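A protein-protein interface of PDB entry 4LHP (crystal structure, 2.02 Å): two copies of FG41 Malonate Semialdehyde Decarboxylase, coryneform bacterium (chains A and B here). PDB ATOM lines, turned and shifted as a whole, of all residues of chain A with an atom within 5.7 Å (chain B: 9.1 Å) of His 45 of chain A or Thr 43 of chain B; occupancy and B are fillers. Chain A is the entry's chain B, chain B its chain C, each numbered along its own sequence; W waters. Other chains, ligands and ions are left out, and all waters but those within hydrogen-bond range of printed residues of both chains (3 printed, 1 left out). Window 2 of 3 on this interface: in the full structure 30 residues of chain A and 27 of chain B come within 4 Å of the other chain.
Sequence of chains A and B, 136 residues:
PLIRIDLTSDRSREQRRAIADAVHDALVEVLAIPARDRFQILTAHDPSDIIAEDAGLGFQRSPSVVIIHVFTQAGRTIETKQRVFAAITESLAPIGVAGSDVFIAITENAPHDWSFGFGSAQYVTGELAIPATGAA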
ATOM      1  N   ASP A   6      -8.204  -7.814 -25.530  1.00  0.00           N
ATOM      2  CA  ASP A   6      -7.366  -6.659 -25.255  1.00  0.00           C
ATOM      3  C   ASP A   6      -5.928  -6.974 -25.638  1.00  0.00           C
ATOM      4  O   ASP A   6      -5.312  -7.890 -25.092  1.00  0.00           O
ATOM      5  CB  ASP A   6      -7.469  -6.272 -23.780  1.00  0.00           C
ATOM      6  CG  ASP A   6      -8.753  -5.527 -23.465  1.00  0.00           C
ATOM      7  OD1 ASP A   6      -8.709  -4.283 -23.364  1.00  0.00           O
ATOM      8  OD2 ASP A   6      -9.807  -6.184 -23.327  1.00  0.00           O
ATOM      9  N   LEU A   7      -5.405  -6.211 -26.590  1.00  0.00           N
ATOM     10  CA  LEU A   7      -4.076  -6.462 -27.129  1.00  0.00           C
ATOM     11  C   LEU A   7      -3.315  -5.147 -27.303  1.00  0.00           C
ATOM     12  O   LEU A   7      -3.774  -4.097 -26.857  1.00  0.00           O
ATOM     13  CB  LEU A   7      -4.188  -7.229 -28.451  1.00  0.00           C
ATOM     14  CG  LEU A   7      -5.273  -6.751 -29.419  1.00  0.00           C
ATOM     15  CD1 LEU A   7      -4.890  -5.424 -30.054  1.00  0.00           C
ATOM     16  CD2 LEU A   7      -5.546  -7.803 -30.485  1.00  0.00           C
ATOM     17  N   THR A   8      -2.152  -5.207 -27.946  1.00  0.00           N
ATOM     18  CA  THR A   8      -1.264  -4.051 -28.011  1.00  0.00           C
ATOM     19  C   THR A   8      -1.310  -3.340 -29.366  1.00  0.00           C
ATOM     20  O   THR A   8      -1.414  -3.971 -30.415  1.00  0.00           O
ATOM     21  CB  THR A   8       0.178  -4.462 -27.682  1.00  0.00           C
ATOM     22  OG1 THR A   8       0.629  -5.441 -28.625  1.00  0.00           O
ATOM     23  CG2 THR A   8       0.244  -5.043 -26.278  1.00  0.00           C
ATOM     24  N   SER A   9      -1.215  -2.013 -29.319  1.00  0.00           N
ATOM     25  CA  SER A   9      -1.421  -1.161 -30.489  1.00  0.00           C
ATOM     26  C   SER A   9      -0.393  -1.355 -31.607  1.00  0.00           C
ATOM     27  O   SER A   9      -0.628  -0.944 -32.744  1.00  0.00           O
ATOM     28  CB  SER A   9      -1.444   0.309 -30.057  1.00  0.00           C
ATOM     29  OG  SER A   9      -0.173   0.731 -29.594  1.00  0.00           O
ATOM     30  N   ASP A  10       0.740  -1.976 -31.295  1.00  0.00           N
ATOM     31  CA  ASP A  10       1.779  -2.181 -32.303  1.00  0.00           C
ATOM     32  C   ASP A  10       1.390  -3.255 -33.317  1.00  0.00           C
ATOM     33  O   ASP A  10       1.932  -3.293 -34.424  1.00  0.00           O
ATOM     34  CB  ASP A  10       3.116  -2.532 -31.647  1.00  0.00           C
ATOM     35  CG  ASP A  10       3.881  -1.304 -31.195  1.00  0.00           C
ATOM     36  OD1 ASP A  10       3.836  -0.279 -31.907  1.00  0.00           O
ATOM     37  OD2 ASP A  10       4.523  -1.360 -30.125  1.00  0.00           O
ATOM     38  N   THR A  43      -9.664  -3.920 -28.034  1.00  0.00           N
ATOM     39  CA  THR A  43      -9.100  -2.703 -27.487  1.00  0.00           C
ATOM     40  C   THR A  43      -7.590  -2.804 -27.535  1.00  0.00           C
ATOM     41  O   THR A  43      -6.999  -3.724 -26.971  1.00  0.00           O
ATOM     42  CB  THR A  43      -9.559  -2.506 -26.047  1.00  0.00           C
ATOM     43  OG1 THR A  43     -10.989  -2.592 -25.992  1.00  0.00           O
ATOM     44  CG2 THR A  43      -9.115  -1.154 -25.531  1.00  0.00           C
ATOM     45  N   ALA A  44      -6.968  -1.856 -28.224  1.00  0.00           N
ATOM     46  CA  ALA A  44      -5.521  -1.837 -28.349  1.00  0.00           C
ATOM     47  C   ALA A  44      -4.931  -0.852 -27.350  1.00  0.00           C
ATOM     48  O   ALA A  44      -5.470   0.234 -27.146  1.00  0.00           O
ATOM     49  CB  ALA A  44      -5.120  -1.465 -29.762  1.00  0.00           C
ATOM     50  N   HIS A  45      -3.832  -1.248 -26.716  1.00  0.00           N
ATOM     51  CA  HIS A  45      -3.160  -0.398 -25.746  1.00  0.00           C
ATOM     52  C   HIS A  45      -1.676  -0.306 -26.054  1.00  0.00           C
ATOM     53  O   HIS A  45      -1.115  -1.171 -26.727  1.00  0.00           O
ATOM     54  CB  HIS A  45      -3.293  -0.972 -24.335  1.00  0.00           C
ATOM     55  CG  HIS A  45      -4.661  -1.469 -23.999  1.00  0.00           C
ATOM     56  ND1 HIS A  45      -5.514  -0.785 -23.160  1.00  0.00           N
ATOM     57  CD2 HIS A  45      -5.320  -2.593 -24.370  1.00  0.00           C
ATOM     58  CE1 HIS A  45      -6.643  -1.462 -23.036  1.00  0.00           C
ATOM     59  NE2 HIS A  45      -6.549  -2.562 -23.763  1.00  0.00           N
ATOM     60  N   ASP A  46      -1.038   0.740 -25.546  1.00  0.00           N
ATOM     61  CA  ASP A  46       0.405   0.726 -25.400  1.00  0.00           C
ATOM     62  C   ASP A  46       0.716  -0.469 -24.509  1.00  0.00           C
ATOM     63  O   ASP A  46       0.007  -0.713 -23.535  1.00  0.00           O
ATOM     64  CB  ASP A  46       0.892   2.013 -24.739  1.00  0.00           C
ATOM     65  CG  ASP A  46       2.402   2.129 -24.737  1.00  0.00           C
ATOM     66  OD1 ASP A  46       2.948   2.779 -25.655  1.00  0.00           O
ATOM     67  OD2 ASP A  46       3.043   1.570 -23.821  1.00  0.00           O
ATOM     68  N   PRO A  47       1.766  -1.233 -24.840  1.00  0.00           N
ATOM     69  CA  PRO A  47       2.056  -2.448 -24.067  1.00  0.00           C
ATOM     70  C   PRO A  47       2.240  -2.193 -22.569  1.00  0.00           C
ATOM     71  O   PRO A  47       2.081  -3.117 -21.771  1.00  0.00           O
ATOM     72  CB  PRO A  47       3.358  -2.954 -24.692  1.00  0.00           C
ATOM     73  CG  PRO A  47       3.334  -2.414 -26.083  1.00  0.00           C
ATOM     74  CD  PRO A  47       2.705  -1.060 -25.961  1.00  0.00           C
ATOM     75  N   ASP A  49       0.320  -0.674 -20.715  1.00  0.00           N
ATOM     76  CA  ASP A  49      -0.988  -0.635 -20.069  1.00  0.00           C
ATOM     77  C   ASP A  49      -1.634  -2.014 -19.994  1.00  0.00           C
ATOM     78  O   ASP A  49      -2.729  -2.163 -19.454  1.00  0.00           O
ATOM     79  CB  ASP A  49      -1.907   0.349 -20.793  1.00  0.00           C
ATOM     80  CG  ASP A  49      -1.435   1.787 -20.665  1.00  0.00           C
ATOM     81  OD1 ASP A  49      -0.807   2.119 -19.635  1.00  0.00           O
ATOM     82  OD2 ASP A  49      -1.691   2.583 -21.593  1.00  0.00           O
ATOM     83  N   ILE A  50      -0.961  -3.019 -20.544  1.00  0.00           N
ATOM     84  CA  ILE A  50      -1.329  -4.401 -20.273  1.00  0.00           C
ATOM     85  C   ILE A  50      -0.216  -5.042 -19.470  1.00  0.00           C
ATOM     86  O   ILE A  50       0.933  -5.102 -19.914  1.00  0.00           O
ATOM     87  CB  ILE A  50      -1.539  -5.235 -21.538  1.00  0.00           C
ATOM     88  CG1 ILE A  50      -2.670  -4.661 -22.391  1.00  0.00           C
ATOM     89  CG2 ILE A  50      -1.871  -6.663 -21.146  1.00  0.00           C
ATOM     90  CD1 ILE A  50      -3.053  -5.552 -23.560  1.00  0.00           C
ATOM     91  N   ILE B   3      -7.661  -7.664 -13.396  1.00  0.00           N
ATOM     92  CA  ILE B   3      -8.171  -6.371 -12.956  1.00  0.00           C
ATOM     93  C   ILE B   3      -8.265  -5.379 -14.103  1.00  0.00           C
ATOM     94  O   ILE B   3      -7.259  -5.041 -14.725  1.00  0.00           O
ATOM     95  CB  ILE B   3      -7.276  -5.750 -11.870  1.00  0.00           C
ATOM     96  CG1 ILE B   3      -6.759  -6.829 -10.914  1.00  0.00           C
ATOM     97  CG2 ILE B   3      -8.038  -4.675 -11.121  1.00  0.00           C
ATOM     98  CD1 ILE B   3      -7.846  -7.584 -10.200  1.00  0.00           C
ATOM     99  N   ARG B   4      -9.477  -4.912 -14.380  1.00  0.00           N
ATOM    100  CA  ARG B   4      -9.668  -3.831 -15.334  1.00  0.00           C
ATOM    101  C   ARG B   4      -9.695  -2.502 -14.597  1.00  0.00           C
ATOM    102  O   ARG B   4     -10.541  -2.271 -13.734  1.00  0.00           O
ATOM    103  CB  ARG B   4     -10.946  -4.040 -16.146  1.00  0.00           C
ATOM    104  CG  ARG B   4     -10.812  -5.202 -17.097  1.00  0.00           C
ATOM    105  CD  ARG B   4     -12.067  -5.522 -17.873  1.00  0.00           C
ATOM    106  NE  ARG B   4     -11.853  -6.771 -18.598  1.00  0.00           N
ATOM    107  CZ  ARG B   4     -11.441  -6.859 -19.860  1.00  0.00           C
ATOM    108  NH1 ARG B   4     -11.228  -5.772 -20.587  1.00  0.00           N
ATOM    109  NH2 ARG B   4     -11.254  -8.046 -20.414  1.00  0.00           N
ATOM    110  N   ILE B   5      -8.738  -1.645 -14.931  1.00  0.00           N
ATOM    111  CA  ILE B   5      -8.636  -0.325 -14.332  1.00  0.00           C
ATOM    112  C   ILE B   5      -8.911   0.734 -15.389  1.00  0.00           C
ATOM    113  O   ILE B   5      -8.090   0.974 -16.274  1.00  0.00           O
ATOM    114  CB  ILE B   5      -7.242  -0.091 -13.741  1.00  0.00           C
ATOM    115  CG1 ILE B   5      -6.965  -1.107 -12.629  1.00  0.00           C
ATOM    116  CG2 ILE B   5      -7.130   1.326 -13.206  1.00  0.00           C
ATOM    117  CD1 ILE B   5      -5.526  -1.135 -12.171  1.00  0.00           C
ATOM    118  N   ASP B   6     -10.079   1.357 -15.296  1.00  0.00           N
ATOM    119  CA  ASP B   6     -10.446   2.430 -16.207  1.00  0.00           C
ATOM    120  C   ASP B   6     -10.319   3.766 -15.489  1.00  0.00           C
ATOM    121  O   ASP B   6     -11.027   4.032 -14.519  1.00  0.00           O
ATOM    122  CB  ASP B   6     -11.866   2.217 -16.730  1.00  0.00           C
ATOM    123  CG  ASP B   6     -11.967   1.023 -17.666  1.00  0.00           C
ATOM    124  OD1 ASP B   6     -11.993   1.229 -18.898  1.00  0.00           O
ATOM    125  OD2 ASP B   6     -12.008  -0.122 -17.170  1.00  0.00           O
ATOM    126  N   LEU B   7      -9.398   4.596 -15.963  1.00  0.00           N
ATOM    127  CA  LEU B   7      -9.144   5.892 -15.347  1.00  0.00           C
ATOM    128  C   LEU B   7      -9.024   6.978 -16.415  1.00  0.00           C
ATOM    129  O   LEU B   7      -9.393   6.758 -17.570  1.00  0.00           O
ATOM    130  CB  LEU B   7      -7.894   5.823 -14.460  1.00  0.00           C
ATOM    131  CG  LEU B   7      -6.743   4.927 -14.925  1.00  0.00           C
ATOM    132  CD1 LEU B   7      -6.186   5.379 -16.261  1.00  0.00           C
ATOM    133  CD2 LEU B   7      -5.649   4.903 -13.868  1.00  0.00           C
ATOM    134  N   THR B   8      -8.522   8.149 -16.035  1.00  0.00           N
ATOM    135  CA  THR B   8      -8.513   9.295 -16.939  1.00  0.00           C
ATOM    136  C   THR B   8      -7.127   9.599 -17.500  1.00  0.00           C
ATOM    137  O   THR B   8      -6.118   9.476 -16.805  1.00  0.00           O
ATOM    138  CB  THR B   8      -9.086  10.545 -16.249  1.00  0.00           C
ATOM    139  OG1 THR B   8      -8.426  10.752 -14.992  1.00  0.00           O
ATOM    140  CG2 THR B   8     -10.572  10.363 -16.002  1.00  0.00           C
ATOM    141  N   SER B   9      -7.095   9.994 -18.770  1.00  0.00           N
ATOM    142  CA  SER B   9      -5.848  10.251 -19.482  1.00  0.00           C
ATOM    143  C   SER B   9      -5.157  11.526 -19.004  1.00  0.00           C
ATOM    144  O   SER B   9      -4.025  11.811 -19.395  1.00  0.00           O
ATOM    145  CB  SER B   9      -6.112  10.336 -20.987  1.00  0.00           C
ATOM    146  OG  SER B   9      -7.134  11.274 -21.273  1.00  0.00           O
ATOM    147  N   ARG B  16      -0.440   6.551 -13.542  1.00  0.00           N
ATOM    148  CA  ARG B  16      -1.290   5.443 -13.963  1.00  0.00           C
ATOM    149  C   ARG B  16      -0.672   4.119 -13.541  1.00  0.00           C
ATOM    150  O   ARG B  16      -1.355   3.247 -13.005  1.00  0.00           O
ATOM    151  CB  ARG B  16      -1.495   5.459 -15.479  1.00  0.00           C
ATOM    152  CG  ARG B  16      -2.562   6.427 -15.950  1.00  0.00           C
ATOM    153  CD  ARG B  16      -2.759   6.341 -17.454  1.00  0.00           C
ATOM    154  NE  ARG B  16      -2.565   7.635 -18.102  1.00  0.00           N
ATOM    155  CZ  ARG B  16      -2.530   7.822 -19.418  1.00  0.00           C
ATOM    156  NH1 ARG B  16      -2.677   6.798 -20.249  1.00  0.00           N
ATOM    157  NH2 ARG B  16      -2.349   9.043 -19.903  1.00  0.00           N
ATOM    158  N   ALA B  20      -1.803   1.251 -10.765  1.00  0.00           N
ATOM    159  CA  ALA B  20      -1.804  -0.182 -11.036  1.00  0.00           C
ATOM    160  C   ALA B  20      -0.979  -0.935  -9.997  1.00  0.00           C
ATOM    161  O   ALA B  20      -1.388  -1.991  -9.513  1.00  0.00           O
ATOM    162  CB  ALA B  20      -1.266  -0.455 -12.429  1.00  0.00           C
ATOM    163  N   GLN B  40      -3.458  -7.100 -15.256  1.00  0.00           N
ATOM    164  CA  GLN B  40      -4.159  -5.829 -15.215  1.00  0.00           C
ATOM    165  C   GLN B  40      -4.262  -5.223 -16.604  1.00  0.00           C
ATOM    166  O   GLN B  40      -3.341  -5.336 -17.413  1.00  0.00           O
ATOM    167  CB  GLN B  40      -3.417  -4.860 -14.295  1.00  0.00           C
ATOM    168  CG  GLN B  40      -3.091  -5.428 -12.924  1.00  0.00           C
ATOM    169  CD  GLN B  40      -2.201  -4.502 -12.115  1.00  0.00           C
ATOM    170  OE1 GLN B  40      -1.257  -3.916 -12.644  1.00  0.00           O
ATOM    171  NE2 GLN B  40      -2.502  -4.359 -10.831  1.00  0.00           N
ATOM    172  N   ILE B  41      -5.394  -4.583 -16.872  1.00  0.00           N
ATOM    173  CA  ILE B  41      -5.588  -3.843 -18.106  1.00  0.00           C
ATOM    174  C   ILE B  41      -5.938  -2.398 -17.779  1.00  0.00           C
ATOM    175  O   ILE B  41      -7.022  -2.107 -17.270  1.00  0.00           O
ATOM    176  CB  ILE B  41      -6.703  -4.457 -18.959  1.00  0.00           C
ATOM    177  CG1 ILE B  41      -6.349  -5.900 -19.320  1.00  0.00           C
ATOM    178  CG2 ILE B  41      -6.919  -3.633 -20.219  1.00  0.00           C
ATOM    179  CD1 ILE B  41      -7.503  -6.687 -19.893  1.00  0.00           C
ATOM    180  N   LEU B  42      -5.006  -1.499 -18.068  1.00  0.00           N
ATOM    181  CA  LEU B  42      -5.199  -0.077 -17.835  1.00  0.00           C
ATOM    182  C   LEU B  42      -5.783   0.579 -19.077  1.00  0.00           C
ATOM    183  O   LEU B  42      -5.159   0.583 -20.139  1.00  0.00           O
ATOM    184  CB  LEU B  42      -3.868   0.584 -17.481  1.00  0.00           C
ATOM    185  CG  LEU B  42      -3.282   0.250 -16.107  1.00  0.00           C
ATOM    186  CD1 LEU B  42      -3.510  -1.209 -15.739  1.00  0.00           C
ATOM    187  CD2 LEU B  42      -1.797   0.576 -16.087  1.00  0.00           C
ATOM    188  N   THR B  43      -6.987   1.123 -18.944  1.00  0.00           N
ATOM    189  CA  THR B  43      -7.624   1.837 -20.040  1.00  0.00           C
ATOM    190  C   THR B  43      -7.862   3.280 -19.621  1.00  0.00           C
ATOM    191  O   THR B  43      -8.638   3.553 -18.706  1.00  0.00           O
ATOM    192  CB  THR B  43      -8.960   1.185 -20.438  1.00  0.00           C
ATOM    193  OG1 THR B  43      -8.732  -0.175 -20.825  1.00  0.00           O
ATOM    194  CG2 THR B  43      -9.599   1.930 -21.594  1.00  0.00           C
ATOM    195  N   ALA B  44      -7.174   4.202 -20.283  1.00  0.00           N
ATOM    196  CA  ALA B  44      -7.328   5.619 -19.992  1.00  0.00           C
ATOM    197  C   ALA B  44      -8.400   6.232 -20.885  1.00  0.00           C
ATOM    198  O   ALA B  44      -8.551   5.851 -22.046  1.00  0.00           O
ATOM    199  CB  ALA B  44      -6.007   6.342 -20.168  1.00  0.00           C
ATOM    200  N   HIS B  45      -9.140   7.183 -20.327  1.00  0.00           N
ATOM    201  CA  HIS B  45     -10.259   7.806 -21.019  1.00  0.00           C
ATOM    202  C   HIS B  45     -10.213   9.312 -20.824  1.00  0.00           C
ATOM    203  O   HIS B  45      -9.621   9.804 -19.865  1.00  0.00           O
ATOM    204  CB  HIS B  45     -11.584   7.306 -20.441  1.00  0.00           C
ATOM    205  CG  HIS B  45     -11.792   5.828 -20.557  1.00  0.00           C
ATOM    206  ND1 HIS B  45     -12.698   5.271 -21.433  1.00  0.00           N
ATOM    207  CD2 HIS B  45     -11.232   4.793 -19.887  1.00  0.00           C
ATOM    208  CE1 HIS B  45     -12.679   3.957 -21.308  1.00  0.00           C
ATOM    209  NE2 HIS B  45     -11.798   3.640 -20.375  1.00  0.00           N
ATOM    210  N   ASP B  46     -10.845  10.049 -21.727  1.00  0.00           N
ATOM    211  CA  ASP B  46     -11.162  11.434 -21.437  1.00  0.00           C
ATOM    212  C   ASP B  46     -12.147  11.385 -20.278  1.00  0.00           C
ATOM    213  O   ASP B  46     -13.005  10.504 -20.237  1.00  0.00           O
ATOM    214  CB  ASP B  46     -11.791  12.125 -22.646  1.00  0.00           C
ATOM    215  CG  ASP B  46     -12.141  13.576 -22.368  1.00  0.00           C
ATOM    216  OD1 ASP B  46     -13.159  13.825 -21.687  1.00  0.00           O
ATOM    217  OD2 ASP B  46     -11.398  14.467 -22.831  1.00  0.00           O
ATOM    218  N   ASP B  49     -15.827  10.496 -20.578  1.00  0.00           N
ATOM    219  CA  ASP B  49     -16.242   9.118 -20.864  1.00  0.00           C
ATOM    220  C   ASP B  49     -16.577   8.321 -19.603  1.00  0.00           C
ATOM    221  O   ASP B  49     -17.288   7.316 -19.668  1.00  0.00           O
ATOM    222  CB  ASP B  49     -15.159   8.383 -21.662  1.00  0.00           C
ATOM    223  CG  ASP B  49     -15.086   8.841 -23.103  1.00  0.00           C
ATOM    224  OD1 ASP B  49     -16.091   9.388 -23.608  1.00  0.00           O
ATOM    225  OD2 ASP B  49     -14.025   8.647 -23.733  1.00  0.00           O
ATOM    226  N   ILE B  50     -16.051   8.755 -18.463  1.00  0.00           N
ATOM    227  CA  ILE B  50     -16.365   8.104 -17.195  1.00  0.00           C
ATOM    228  C   ILE B  50     -17.362   8.933 -16.395  1.00  0.00           C
ATOM    229  O   ILE B  50     -17.067  10.053 -15.983  1.00  0.00           O
ATOM    230  CB  ILE B  50     -15.110   7.874 -16.338  1.00  0.00           C
ATOM    231  CG1 ILE B  50     -14.102   7.009 -17.097  1.00  0.00           C
ATOM    232  CG2 ILE B  50     -15.491   7.218 -15.018  1.00  0.00           C
ATOM    233  CD1 ILE B  50     -12.870   6.648 -16.288  1.00  0.00           C
ATOM    234  N   VAL B  65     -11.822  10.201 -11.857  1.00  0.00           N
ATOM    235  CA  VAL B  65     -12.316   8.968 -11.261  1.00  0.00           C
ATOM    236  C   VAL B  65     -11.393   7.808 -11.608  1.00  0.00           C
ATOM    237  O   VAL B  65     -10.762   7.797 -12.665  1.00  0.00           O
ATOM    238  CB  VAL B  65     -13.741   8.629 -11.758  1.00  0.00           C
ATOM    239  CG1 VAL B  65     -14.221   7.300 -11.180  1.00  0.00           C
ATOM    240  CG2 VAL B  65     -14.715   9.738 -11.400  1.00  0.00           C
ATOM    241  N   VAL B  66     -11.302   6.842 -10.701  1.00  0.00           N
ATOM    242  CA  VAL B  66     -10.636   5.584 -10.988  1.00  0.00           C
ATOM    243  C   VAL B  66     -11.586   4.430 -10.715  1.00  0.00           C
ATOM    244  O   VAL B  66     -11.997   4.208  -9.577  1.00  0.00           O
ATOM    245  CB  VAL B  66      -9.376   5.396 -10.133  1.00  0.00           C
ATOM    246  CG1 VAL B  66      -8.774   4.020 -10.388  1.00  0.00           C
ATOM    247  CG2 VAL B  66      -8.368   6.494 -10.426  1.00  0.00           C
ATOM    248  N   ILE B  67     -11.933   3.693 -11.762  1.00  0.00           N
ATOM    249  CA  ILE B  67     -12.796   2.535 -11.612  1.00  0.00           C
ATOM    250  C   ILE B  67     -11.968   1.260 -11.681  1.00  0.00           C
ATOM    251  O   ILE B  67     -11.207   1.045 -12.625  1.00  0.00           O
ATOM    252  CB  ILE B  67     -13.903   2.513 -12.678  1.00  0.00           C
ATOM    253  CG1 ILE B  67     -14.709   3.815 -12.602  1.00  0.00           C
ATOM    254  CG2 ILE B  67     -14.797   1.291 -12.486  1.00  0.00           C
ATOM    255  CD1 ILE B  67     -16.137   3.701 -13.086  1.00  0.00           C
HETATM  256  O   HOH W   1      -4.020   1.657 -22.529  1.00  0.00           O
HETATM  257  O   HOH W   2      -9.753  -8.627 -22.398  1.00  0.00           O
HETATM  258  O   HOH W   3     -10.743  -1.974 -22.678  1.00  0.00           O
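Ile 41 of chain B touches Asp 6 of chain A (CG2 to OD1, 3.7 Å).
Ile 41 of chain B touches His 45 of chain A (CG2 to CE1, 3.6 Å).
His 45 of chain A touches Thr 43 of chain B.
Asp 49 of chain A touches Gln 40 of chain B.
CA of Ile 41 of chain B touches O of Asp 49 of chain A, at 3.6 Å.
O of Gln 40 of chain B touches CA of Ile 50 of chain A (3.6 Å).
The side-chain carboxylate (OD2) of Asp 6 of chain A is in salt-bridge range of the guanidinium group (NH1) of Arg 4 of chain B (3.1 Å).
O of Leu 42 of chain B sits at hydrogen-bond distance from ND1 of His 45 of chain A (3.3 Å).
The backbone NH (N) of Leu 42 of chain B lies within hydrogen-bond range of the backbone carbonyl oxygen (O) of Asp 49 of chain A, at 2.7 Å.
The backbone carbonyl oxygen of Leu 7 of chain A sits at hydrogen-bond distance from the backbone NH of His 45 of chain A (2.9 Å).
N of Ser 9 of chain A lies within hydrogen-bond range of O of His 45 of chain A (2.7 Å).
A ring nitrogen (NE2) of His 45 of chain A sits close to the backbone carbonyl oxygen (O) of Thr 43 of chain A, at 3.4 Å.
The backbone carbonyl oxygen of Ile 3 of chain B is in hydrogen-bond range of the backbone NH of Ile 41 of chain B (2.9 Å).
N of Thr 43 of chain B lies within hydrogen-bond range of O of Ile 5 of chain B (2.9 Å).
The backbone carbonyl oxygen (O) of Thr 43 of chain B is in hydrogen-bond range of the backbone NH (N) of Leu 7 of chain B, 3.0 Å away.
His 45 of chain A touches Thr 43 of chain B, but with the chains exchanged Thr 43 of chain A does not touch His 45 of chain B (7.5 Å).
Positions printed for both chains: 6, 7, 8, 9, 43, 44, 45, 46, 49 and 50.
Of the 9 pairs that touch across the chains among the printed residues, none has its exchanged pair printed and touching as well.
Water W2 bridges NH2 of Arg 4 of chain B (2.6 Å) and OD2 of Asp 6 of chain A (2.6 Å).
Water W1 lies within hydrogen-bond range of OD2 of Asp 49 of chain A, O of Leu 42 of chain B and ND1 of His 45 of chain A.
Water W3 lies within hydrogen-bond range of the side-chain carboxylate of Asp 6 of chain A (3.2 Å), the side-chain hydroxyl of Thr 43 of chain B (3.3 Å) and the side-chain hydroxyl of Thr 43 of chain A (3.4 Å).
No residue of chain B comes within 4 Å of Thr 8 of chain A.
Of chain B, only Ile 41, Leu 42 and Thr 43 come within 4 Å of His 45 of chain A.
Printed residues of chain B within 4 Å of Asp 49 of chain A: Gln 40, Ile 41 and Leu 42.
Of the printed residues of chain A, Gln 40 of chain B touches Asp 49 (3.8 Å) and Ile 50 (3.6 Å).
His 45 of chain B touches none of the printed residues of chain A.
The nearest printed residue of chain A that does not touch Thr 43 of chain B is Thr 43 of chain A (4.8 Å).
Printed residues of chain A that touch a printed residue of chain B: Asp 6, His 45, Asp 49 and Ile 50.
Of the 21 printed residues of chain B, 5 touch a printed residue of chain A.
Hydrophobic or aromatic side chains of chain B within 4 Å of the printed part of chain A: Ile 41 and Leu 42.
Among the printed residues, Asp or Glu carboxylates within 4 Å of a Lys or Arg side-chain nitrogen of the other chain: Asp 6 of chain A with Arg 4 of chain B (3.1 Å).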
